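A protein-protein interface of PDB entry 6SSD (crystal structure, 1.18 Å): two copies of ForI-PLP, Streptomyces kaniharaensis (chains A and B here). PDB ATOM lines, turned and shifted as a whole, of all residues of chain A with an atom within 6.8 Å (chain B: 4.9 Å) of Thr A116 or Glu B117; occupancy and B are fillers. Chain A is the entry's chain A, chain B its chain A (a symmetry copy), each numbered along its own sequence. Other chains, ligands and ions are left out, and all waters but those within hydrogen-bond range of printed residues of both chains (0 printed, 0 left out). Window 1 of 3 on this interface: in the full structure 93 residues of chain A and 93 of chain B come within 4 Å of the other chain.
CB of Thr A116 touches OE1 of Glu B117, 3.8 Å away. Thr B116 touches Glu A117 (CB to OE1, 3.8 Å). SD of Met B121 touches CB of Ala A145 (3.9 Å). Tyr A146 touches Met B120.
The side-chain carboxylate of Glu A117 lies within hydrogen-bond range of the side-chain hydroxyl of Ser B114 (2.6 Å). The side-chain carboxylate (OE1) of Glu B117 lies within hydrogen-bond range of the side-chain hydroxyl (OG) of Ser A114 (2.6 Å).
Of the 20 printed residues of chain A, 5 touch a printed residue of chain B. Printed residues of chain A that touch a printed residue of chain B: Ser A114, Thr A116, Glu A117, Ala A145 and Tyr A146. Printed residues of chain B that touch a printed residue of chain A: Ser B114, Thr B116, Glu B117, Met B120 and Met B121. Hydrophobic or aromatic side chains of chain B within 4 Å of the printed part of chain A: Met B120 and Met B121. Along chain B the printed residues that touch a printed residue of chain A span positions 114 to 121. Among the printed residues, 6 pairs touch across the chains.
Ser A114 touches Glu B117, and with the chains exchanged Glu A117 touches Ser B114. Thr A116 touches Glu B117, and with the chains exchanged Glu A117 touches Thr B116. Positions printed for both chains: 112, 113, 114, 115, 116, 117, 118, 119, 120 and 121.
N of Thr A116 sits close to OG of Ser A114, at 3.4 Å. The backbone NH (N) of Ser B113 is in hydrogen-bond range of the side-chain carboxylate (OE2) of Glu B117. The backbone NH of Ser A113 lies within hydrogen-bond range of the side-chain carboxylate of Glu A117, at 2.9 Å. OG of Ser B114 sits close to N of Thr B116 (3.4 Å). The side-chain hydroxyl (OG1) of Thr B112 sits at hydrogen-bond distance from the backbone carbonyl oxygen (O) of Ser B114 (2.8 Å). The backbone NH of Glu B117 sits at hydrogen-bond distance from the side-chain hydroxyl of Ser B114 (3.0 Å).
Of chain B, only Glu B117 comes within 4 Å of Thr A116. Of chain A, only Ser A114 (2.6 Å) and Thr A116 (3.8 Å) come within 4 Å of Glu B117. Of the printed residues of chain A, Met B120 touches Tyr A146 (3.8 Å). Printed residues of chain A within 4 Å of Thr B116: Glu A117 (3.8 Å). The nearest residue of chain B that does not touch Thr A116 is Met B120 (4.2 Å). The nearest printed residue of chain A that does not touch Met B121 is Tyr A146 (6.1 Å).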
ATOM      1  N   THR A 112      -1.683 -16.099 -22.433  1.00  0.00           N
ATOM      2  CA  THR A 112      -1.708 -17.467 -22.920  1.00  0.00           C
ATOM      3  C   THR A 112      -0.716 -18.291 -22.110  1.00  0.00           C
ATOM      4  O   THR A 112      -0.013 -17.759 -21.225  1.00  0.00           O
ATOM      5  CB  THR A 112      -1.320 -17.497 -24.409  1.00  0.00           C
ATOM      6  OG1 THR A 112       0.030 -17.092 -24.505  1.00  0.00           O
ATOM      7  CG2 THR A 112      -2.183 -16.593 -25.262  1.00  0.00           C
ATOM      8  N   SER A 113      -0.580 -19.575 -22.445  1.00  0.00           N
ATOM      9  CA  SER A 113       0.402 -20.449 -21.788  1.00  0.00           C
ATOM     10  C   SER A 113       1.732 -20.592 -22.487  1.00  0.00           C
ATOM     11  O   SER A 113       2.633 -21.259 -21.981  1.00  0.00           O
ATOM     12  CB  SER A 113      -0.209 -21.801 -21.465  1.00  0.00           C
ATOM     13  OG  SER A 113      -1.130 -21.672 -20.387  1.00  0.00           O
ATOM     14  N   SER A 114       1.873 -19.967 -23.657  1.00  0.00           N
ATOM     15  CA  SER A 114       3.108 -20.025 -24.405  1.00  0.00           C
ATOM     16  C   SER A 114       3.154 -18.917 -25.445  1.00  0.00           C
ATOM     17  O   SER A 114       2.102 -18.361 -25.836  1.00  0.00           O
ATOM     18  CB  SER A 114       3.265 -21.361 -25.111  1.00  0.00           C
ATOM     19  OG  SER A 114       2.280 -21.465 -26.142  1.00  0.00           O
ATOM     20  N   GLY A 115       4.360 -18.600 -25.892  1.00  0.00           N
ATOM     21  CA  GLY A 115       4.505 -17.699 -27.031  1.00  0.00           C
ATOM     22  C   GLY A 115       3.892 -18.255 -28.291  1.00  0.00           C
ATOM     23  O   GLY A 115       3.358 -17.516 -29.113  1.00  0.00           O
ATOM     24  N   THR A 116       3.974 -19.581 -28.454  1.00  0.00           N
ATOM     25  CA  THR A 116       3.367 -20.237 -29.615  1.00  0.00           C
ATOM     26  C   THR A 116       1.865 -19.945 -29.686  1.00  0.00           C
ATOM     27  O   THR A 116       1.362 -19.613 -30.765  1.00  0.00           O
ATOM     28  CB  THR A 116       3.674 -21.745 -29.525  1.00  0.00           C
ATOM     29  OG1 THR A 116       5.089 -21.927 -29.699  1.00  0.00           O
ATOM     30  CG2 THR A 116       2.913 -22.574 -30.524  1.00  0.00           C
ATOM     31  N   GLU A 117       1.189 -20.128 -28.559  1.00  0.00           N
ATOM     32  CA  GLU A 117      -0.236 -19.802 -28.491  1.00  0.00           C
ATOM     33  C   GLU A 117      -0.490 -18.316 -28.730  1.00  0.00           C
ATOM     34  O   GLU A 117      -1.473 -17.950 -29.370  1.00  0.00           O
ATOM     35  CB  GLU A 117      -0.830 -20.166 -27.129  1.00  0.00           C
ATOM     36  CG  GLU A 117      -1.084 -21.607 -26.845  1.00  0.00           C
ATOM     37  CD  GLU A 117      -1.806 -21.863 -25.491  1.00  0.00           C
ATOM     38  OE1 GLU A 117      -2.249 -22.995 -25.302  1.00  0.00           O
ATOM     39  OE2 GLU A 117      -1.922 -20.909 -24.657  1.00  0.00           O
ATOM     40  N   ALA A 118       0.365 -17.469 -28.138  1.00  0.00           N
ATOM     41  CA  ALA A 118       0.162 -16.024 -28.278  1.00  0.00           C
ATOM     42  C   ALA A 118       0.286 -15.562 -29.739  1.00  0.00           C
ATOM     43  O   ALA A 118      -0.494 -14.737 -30.202  1.00  0.00           O
ATOM     44  CB  ALA A 118       1.089 -15.280 -27.343  1.00  0.00           C
ATOM     45  N   VAL A 119       1.287 -16.102 -30.444  1.00  0.00           N
ATOM     46  CA  VAL A 119       1.393 -15.749 -31.868  1.00  0.00           C
ATOM     47  C   VAL A 119       0.144 -16.188 -32.619  1.00  0.00           C
ATOM     48  O   VAL A 119      -0.405 -15.444 -33.452  1.00  0.00           O
ATOM     49  CB  VAL A 119       2.642 -16.389 -32.505  1.00  0.00           C
ATOM     50  CG1 VAL A 119       2.600 -16.285 -34.035  1.00  0.00           C
ATOM     51  CG2 VAL A 119       3.931 -15.832 -31.974  1.00  0.00           C
ATOM     52  N   MET A 120      -0.304 -17.411 -32.352  1.00  0.00           N
ATOM     53  CA  MET A 120      -1.522 -17.922 -32.990  1.00  0.00           C
ATOM     54  C   MET A 120      -2.708 -16.986 -32.719  1.00  0.00           C
ATOM     55  O   MET A 120      -3.445 -16.645 -33.657  1.00  0.00           O
ATOM     56  CB  MET A 120      -1.807 -19.346 -32.526  1.00  0.00           C
ATOM     57  CG  MET A 120      -3.067 -19.943 -33.137  1.00  0.00           C
ATOM     58  SD  MET A 120      -3.332 -21.661 -32.761  1.00  0.00           S
ATOM     59  CE  MET A 120      -3.923 -21.552 -31.075  1.00  0.00           C
ATOM     60  N   MET A 121      -2.881 -16.587 -31.460  1.00  0.00           N
ATOM     61  CA  MET A 121      -4.030 -15.742 -31.158  1.00  0.00           C
ATOM     62  C   MET A 121      -3.906 -14.341 -31.752  1.00  0.00           C
ATOM     63  O   MET A 121      -4.930 -13.730 -32.095  1.00  0.00           O
ATOM     64  CB  MET A 121      -4.291 -15.707 -29.659  1.00  0.00           C
ATOM     65  CG  MET A 121      -4.611 -17.072 -29.041  1.00  0.00           C
ATOM     66  SD  MET A 121      -5.741 -18.122 -29.941  1.00  0.00           S
ATOM     67  CE  MET A 121      -7.232 -17.132 -29.924  1.00  0.00           C
ATOM     68  N   TYR A 142      11.360 -17.503 -37.215  1.00  0.00           N
ATOM     69  CA  TYR A 142      10.604 -18.492 -36.435  1.00  0.00           C
ATOM     70  C   TYR A 142       9.622 -17.852 -35.504  1.00  0.00           C
ATOM     71  O   TYR A 142       9.953 -16.874 -34.821  1.00  0.00           O
ATOM     72  CB  TYR A 142      11.553 -19.311 -35.575  1.00  0.00           C
ATOM     73  CG  TYR A 142      10.929 -20.204 -34.490  1.00  0.00           C
ATOM     74  CD1 TYR A 142      10.477 -21.489 -34.781  1.00  0.00           C
ATOM     75  CD2 TYR A 142      10.842 -19.777 -33.169  1.00  0.00           C
ATOM     76  CE1 TYR A 142       9.979 -22.322 -33.789  1.00  0.00           C
ATOM     77  CE2 TYR A 142      10.338 -20.589 -32.182  1.00  0.00           C
ATOM     78  CZ  TYR A 142       9.917 -21.866 -32.499  1.00  0.00           C
ATOM     79  OH  TYR A 142       9.419 -22.729 -31.555  1.00  0.00           O
ATOM     80  N   HIS A 143       8.438 -18.457 -35.405  1.00  0.00           N
ATOM     81  CA  HIS A 143       7.368 -17.992 -34.547  1.00  0.00           C
ATOM     82  C   HIS A 143       6.637 -19.108 -33.817  1.00  0.00           C
ATOM     83  O   HIS A 143       5.542 -18.882 -33.342  1.00  0.00           O
ATOM     84  CB  HIS A 143       6.341 -17.152 -35.346  1.00  0.00           C
ATOM     85  CG  HIS A 143       6.937 -15.999 -36.074  1.00  0.00           C
ATOM     86  ND1 HIS A 143       7.188 -14.776 -35.488  1.00  0.00           N
ATOM     87  CD2 HIS A 143       7.299 -15.863 -37.382  1.00  0.00           C
ATOM     88  CE1 HIS A 143       7.721 -13.966 -36.400  1.00  0.00           C
ATOM     89  NE2 HIS A 143       7.799 -14.597 -37.561  1.00  0.00           N
ATOM     90  N   GLY A 144       7.250 -20.284 -33.756  1.00  0.00           N
ATOM     91  CA  GLY A 144       6.612 -21.455 -33.159  1.00  0.00           C
ATOM     92  C   GLY A 144       5.888 -22.322 -34.177  1.00  0.00           C
ATOM     93  O   GLY A 144       5.907 -22.073 -35.387  1.00  0.00           O
ATOM     94  N   ALA A 145       5.204 -23.347 -33.665  1.00  0.00           N
ATOM     95  CA  ALA A 145       4.705 -24.438 -34.506  1.00  0.00           C
ATOM     96  C   ALA A 145       3.345 -24.198 -35.112  1.00  0.00           C
ATOM     97  O   ALA A 145       2.890 -25.005 -35.931  1.00  0.00           O
ATOM     98  CB  ALA A 145       4.681 -25.724 -33.701  1.00  0.00           C
ATOM     99  N   TYR A 146       2.643 -23.113 -34.767  1.00  0.00           N
ATOM    100  CA  TYR A 146       1.318 -22.896 -35.369  1.00  0.00           C
ATOM    101  C   TYR A 146       1.439 -22.893 -36.894  1.00  0.00           C
ATOM    102  O   TYR A 146       2.318 -22.237 -37.484  1.00  0.00           O
ATOM    103  CB  TYR A 146       0.730 -21.578 -34.846  1.00  0.00           C
ATOM    104  CG  TYR A 146      -0.463 -21.027 -35.596  1.00  0.00           C
ATOM    105  CD1 TYR A 146      -1.563 -21.769 -35.901  1.00  0.00           C
ATOM    106  CD2 TYR A 146      -0.462 -19.694 -35.977  1.00  0.00           C
ATOM    107  CE1 TYR A 146      -2.639 -21.225 -36.603  1.00  0.00           C
ATOM    108  CE2 TYR A 146      -1.529 -19.139 -36.633  1.00  0.00           C
ATOM    109  CZ  TYR A 146      -2.601 -19.894 -36.963  1.00  0.00           C
ATOM    110  OH  TYR A 146      -3.639 -19.275 -37.638  1.00  0.00           O
ATOM    111  N   VAL A 149       2.255 -19.937 -39.357  1.00  0.00           N
ATOM    112  CA  VAL A 149       3.529 -19.274 -39.197  1.00  0.00           C
ATOM    113  C   VAL A 149       4.717 -20.216 -39.275  1.00  0.00           C
ATOM    114  O   VAL A 149       5.868 -19.765 -39.235  1.00  0.00           O
ATOM    115  CB  VAL A 149       3.596 -18.415 -37.904  1.00  0.00           C
ATOM    116  CG1 VAL A 149       2.472 -17.375 -37.876  1.00  0.00           C
ATOM    117  CG2 VAL A 149       3.544 -19.290 -36.649  1.00  0.00           C
ATOM    118  N   VAL A 238       8.497 -12.263 -28.619  1.00  0.00           N
ATOM    119  CA  VAL A 238       8.636 -13.320 -27.595  1.00  0.00           C
ATOM    120  C   VAL A 238      10.112 -13.477 -27.225  1.00  0.00           C
ATOM    121  O   VAL A 238      10.425 -13.628 -26.049  1.00  0.00           O
ATOM    122  CB  VAL A 238       7.964 -14.628 -28.049  1.00  0.00           C
ATOM    123  CG1 VAL A 238       8.244 -15.711 -27.046  1.00  0.00           C
ATOM    124  CG2 VAL A 238       6.467 -14.434 -28.176  1.00  0.00           C
ATOM    125  N   VAL A 260       3.440  -9.448 -29.534  1.00  0.00           N
ATOM    126  CA  VAL A 260       3.404 -10.773 -28.910  1.00  0.00           C
ATOM    127  C   VAL A 260       4.613 -10.858 -27.971  1.00  0.00           C
ATOM    128  O   VAL A 260       5.739 -10.501 -28.367  1.00  0.00           O
ATOM    129  CB  VAL A 260       3.471 -11.925 -29.926  1.00  0.00           C
ATOM    130  CG1 VAL A 260       3.074 -13.224 -29.278  1.00  0.00           C
ATOM    131  CG2 VAL A 260       2.597 -11.664 -31.143  1.00  0.00           C
ATOM    132  N   ILE A 271       4.143 -18.992 -20.116  1.00  0.00           N
ATOM    133  CA  ILE A 271       3.358 -17.798 -20.392  1.00  0.00           C
ATOM    134  C   ILE A 271       3.531 -17.379 -21.844  1.00  0.00           C
ATOM    135  O   ILE A 271       4.534 -17.705 -22.488  1.00  0.00           O
ATOM    136  CB  ILE A 271       3.777 -16.624 -19.465  1.00  0.00           C
ATOM    137  CG1 ILE A 271       2.658 -15.605 -19.290  1.00  0.00           C
ATOM    138  CG2 ILE A 271       5.057 -15.959 -19.918  1.00  0.00           C
ATOM    139  CD1 ILE A 271       2.920 -14.625 -18.167  1.00  0.00           C
ATOM    140  N   GLY A 272       2.556 -16.587 -22.286  1.00  0.00           N
ATOM    141  CA  GLY A 272       2.648 -15.750 -23.463  1.00  0.00           C
ATOM    142  C   GLY A 272       1.697 -14.588 -23.256  1.00  0.00           C
ATOM    143  O   GLY A 272       0.827 -14.637 -22.357  1.00  0.00           O
ATOM    144  N   THR B 112       3.569 -30.921 -24.198  1.00  0.00           N
ATOM    145  CA  THR B 112       3.312 -29.548 -24.594  1.00  0.00           C
ATOM    146  C   THR B 112       2.974 -28.736 -23.351  1.00  0.00           C
ATOM    147  O   THR B 112       2.911 -29.281 -22.227  1.00  0.00           O
ATOM    148  CB  THR B 112       2.134 -29.502 -25.584  1.00  0.00           C
ATOM    149  OG1 THR B 112       0.976 -29.911 -24.885  1.00  0.00           O
ATOM    150  CG2 THR B 112       2.341 -30.394 -26.789  1.00  0.00           C
ATOM    151  N   SER B 113       2.674 -27.449 -23.531  1.00  0.00           N
ATOM    152  CA  SER B 113       2.256 -26.586 -22.416  1.00  0.00           C
ATOM    153  C   SER B 113       0.768 -26.440 -22.216  1.00  0.00           C
ATOM    154  O   SER B 113       0.328 -25.782 -21.274  1.00  0.00           O
ATOM    155  CB  SER B 113       2.946 -25.236 -22.492  1.00  0.00           C
ATOM    156  OG  SER B 113       4.321 -25.373 -22.147  1.00  0.00           O
ATOM    157  N   SER B 114      -0.027 -27.052 -23.096  1.00  0.00           N
ATOM    158  CA  SER B 114      -1.467 -26.991 -22.990  1.00  0.00           C
ATOM    159  C   SER B 114      -2.110 -28.087 -23.825  1.00  0.00           C
ATOM    160  O   SER B 114      -1.479 -28.634 -24.758  1.00  0.00           O
ATOM    161  CB  SER B 114      -1.998 -25.647 -23.460  1.00  0.00           C
ATOM    162  OG  SER B 114      -1.790 -25.528 -24.869  1.00  0.00           O
ATOM    163  N   GLY B 115      -3.353 -28.403 -23.495  1.00  0.00           N
ATOM    164  CA  GLY B 115      -4.133 -29.291 -24.349  1.00  0.00           C
ATOM    165  C   GLY B 115      -4.360 -28.719 -25.725  1.00  0.00           C
ATOM    166  O   GLY B 115      -4.404 -29.447 -26.713  1.00  0.00           O
ATOM    167  N   THR B 116      -4.517 -27.392 -25.796  1.00  0.00           N
ATOM    168  CA  THR B 116      -4.691 -26.721 -27.086  1.00  0.00           C
ATOM    169  C   THR B 116      -3.509 -27.007 -28.017  1.00  0.00           C
ATOM    170  O   THR B 116      -3.724 -27.325 -29.192  1.00  0.00           O
ATOM    171  CB  THR B 116      -4.884 -25.216 -26.819  1.00  0.00           C
ATOM    172  OG1 THR B 116      -6.139 -25.036 -26.140  1.00  0.00           O
ATOM    173  CG2 THR B 116      -4.839 -24.372 -28.065  1.00  0.00           C
ATOM    174  N   GLU B 117      -2.305 -26.834 -27.487  1.00  0.00           N
ATOM    175  CA  GLU B 117      -1.104 -27.156 -28.260  1.00  0.00           C
ATOM    176  C   GLU B 117      -1.040 -28.638 -28.619  1.00  0.00           C
ATOM    177  O   GLU B 117      -0.610 -28.993 -29.713  1.00  0.00           O
ATOM    178  CB  GLU B 117       0.169 -26.805 -27.489  1.00  0.00           C
ATOM    179  CG  GLU B 117       0.546 -25.366 -27.388  1.00  0.00           C
ATOM    180  CD  GLU B 117       1.920 -25.123 -26.699  1.00  0.00           C
ATOM    181  OE1 GLU B 117       2.394 -23.992 -26.788  1.00  0.00           O
ATOM    182  OE2 GLU B 117       2.493 -26.085 -26.096  1.00  0.00           O
ATOM    183  N   ALA B 118      -1.398 -29.495 -27.651  1.00  0.00           N
ATOM    184  CA  ALA B 118      -1.319 -30.937 -27.898  1.00  0.00           C
ATOM    185  C   ALA B 118      -2.267 -31.383 -29.023  1.00  0.00           C
ATOM    186  O   ALA B 118      -1.902 -32.200 -29.861  1.00  0.00           O
ATOM    187  CB  ALA B 118      -1.536 -31.695 -26.607  1.00  0.00           C
ATOM    188  N   VAL B 119      -3.490 -30.839 -29.013  1.00  0.00           N
ATOM    189  CA  VAL B 119      -4.401 -31.176 -30.116  1.00  0.00           C
ATOM    190  C   VAL B 119      -3.815 -30.724 -31.447  1.00  0.00           C
ATOM    191  O   VAL B 119      -3.852 -31.457 -32.452  1.00  0.00           O
ATOM    192  CB  VAL B 119      -5.786 -30.533 -29.906  1.00  0.00           C
ATOM    193  CG1 VAL B 119      -6.637 -30.620 -31.179  1.00  0.00           C
ATOM    194  CG2 VAL B 119      -6.532 -31.101 -28.733  1.00  0.00           C
ATOM    195  N   MET B 120      -3.291 -29.503 -31.474  1.00  0.00           N
ATOM    196  CA  MET B 120      -2.665 -28.980 -32.694  1.00  0.00           C
ATOM    197  C   MET B 120      -1.544 -29.916 -33.170  1.00  0.00           C
ATOM    198  O   MET B 120      -1.487 -30.243 -34.365  1.00  0.00           O
ATOM    199  CB  MET B 120      -2.159 -27.561 -32.464  1.00  0.00           C
ATOM    200  CG  MET B 120      -1.483 -26.952 -33.686  1.00  0.00           C
ATOM    201  SD  MET B 120      -1.043 -25.238 -33.512  1.00  0.00           S
ATOM    202  CE  MET B 120       0.414 -25.363 -32.480  1.00  0.00           C
ATOM    203  N   MET B 121      -0.677 -30.328 -32.247  1.00  0.00           N
ATOM    204  CA  MET B 121       0.432 -31.171 -32.675  1.00  0.00           C
ATOM    205  C   MET B 121      -0.017 -32.566 -33.104  1.00  0.00           C
ATOM    206  O   MET B 121       0.617 -33.170 -33.983  1.00  0.00           O
ATOM    207  CB  MET B 121       1.512 -31.222 -31.604  1.00  0.00           C
ATOM    208  CG  MET B 121       2.136 -29.864 -31.270  1.00  0.00           C
ATOM    209  SD  MET B 121       2.541 -28.800 -32.647  1.00  0.00           S
ATOM    210  CE  MET B 121       3.763 -29.785 -33.506  1.00  0.00           C
ATOM    211  N   ASN B 300       8.086 -27.001 -22.835  1.00  0.00           N
ATOM    212  CA  ASN B 300       7.804 -28.402 -23.033  1.00  0.00           C
ATOM    213  C   ASN B 300       8.616 -29.212 -22.017  1.00  0.00           C
ATOM    214  O   ASN B 300       9.846 -29.046 -21.922  1.00  0.00           O
ATOM    215  CB  ASN B 300       8.260 -28.889 -24.398  1.00  0.00           C
ATOM    216  CG  ASN B 300       7.493 -28.379 -25.594  1.00  0.00           C
ATOM    217  OD1 ASN B 300       6.711 -27.441 -25.484  1.00  0.00           O
ATOM    218  ND2 ASN B 300       7.764 -28.979 -26.759  1.00  0.00           N
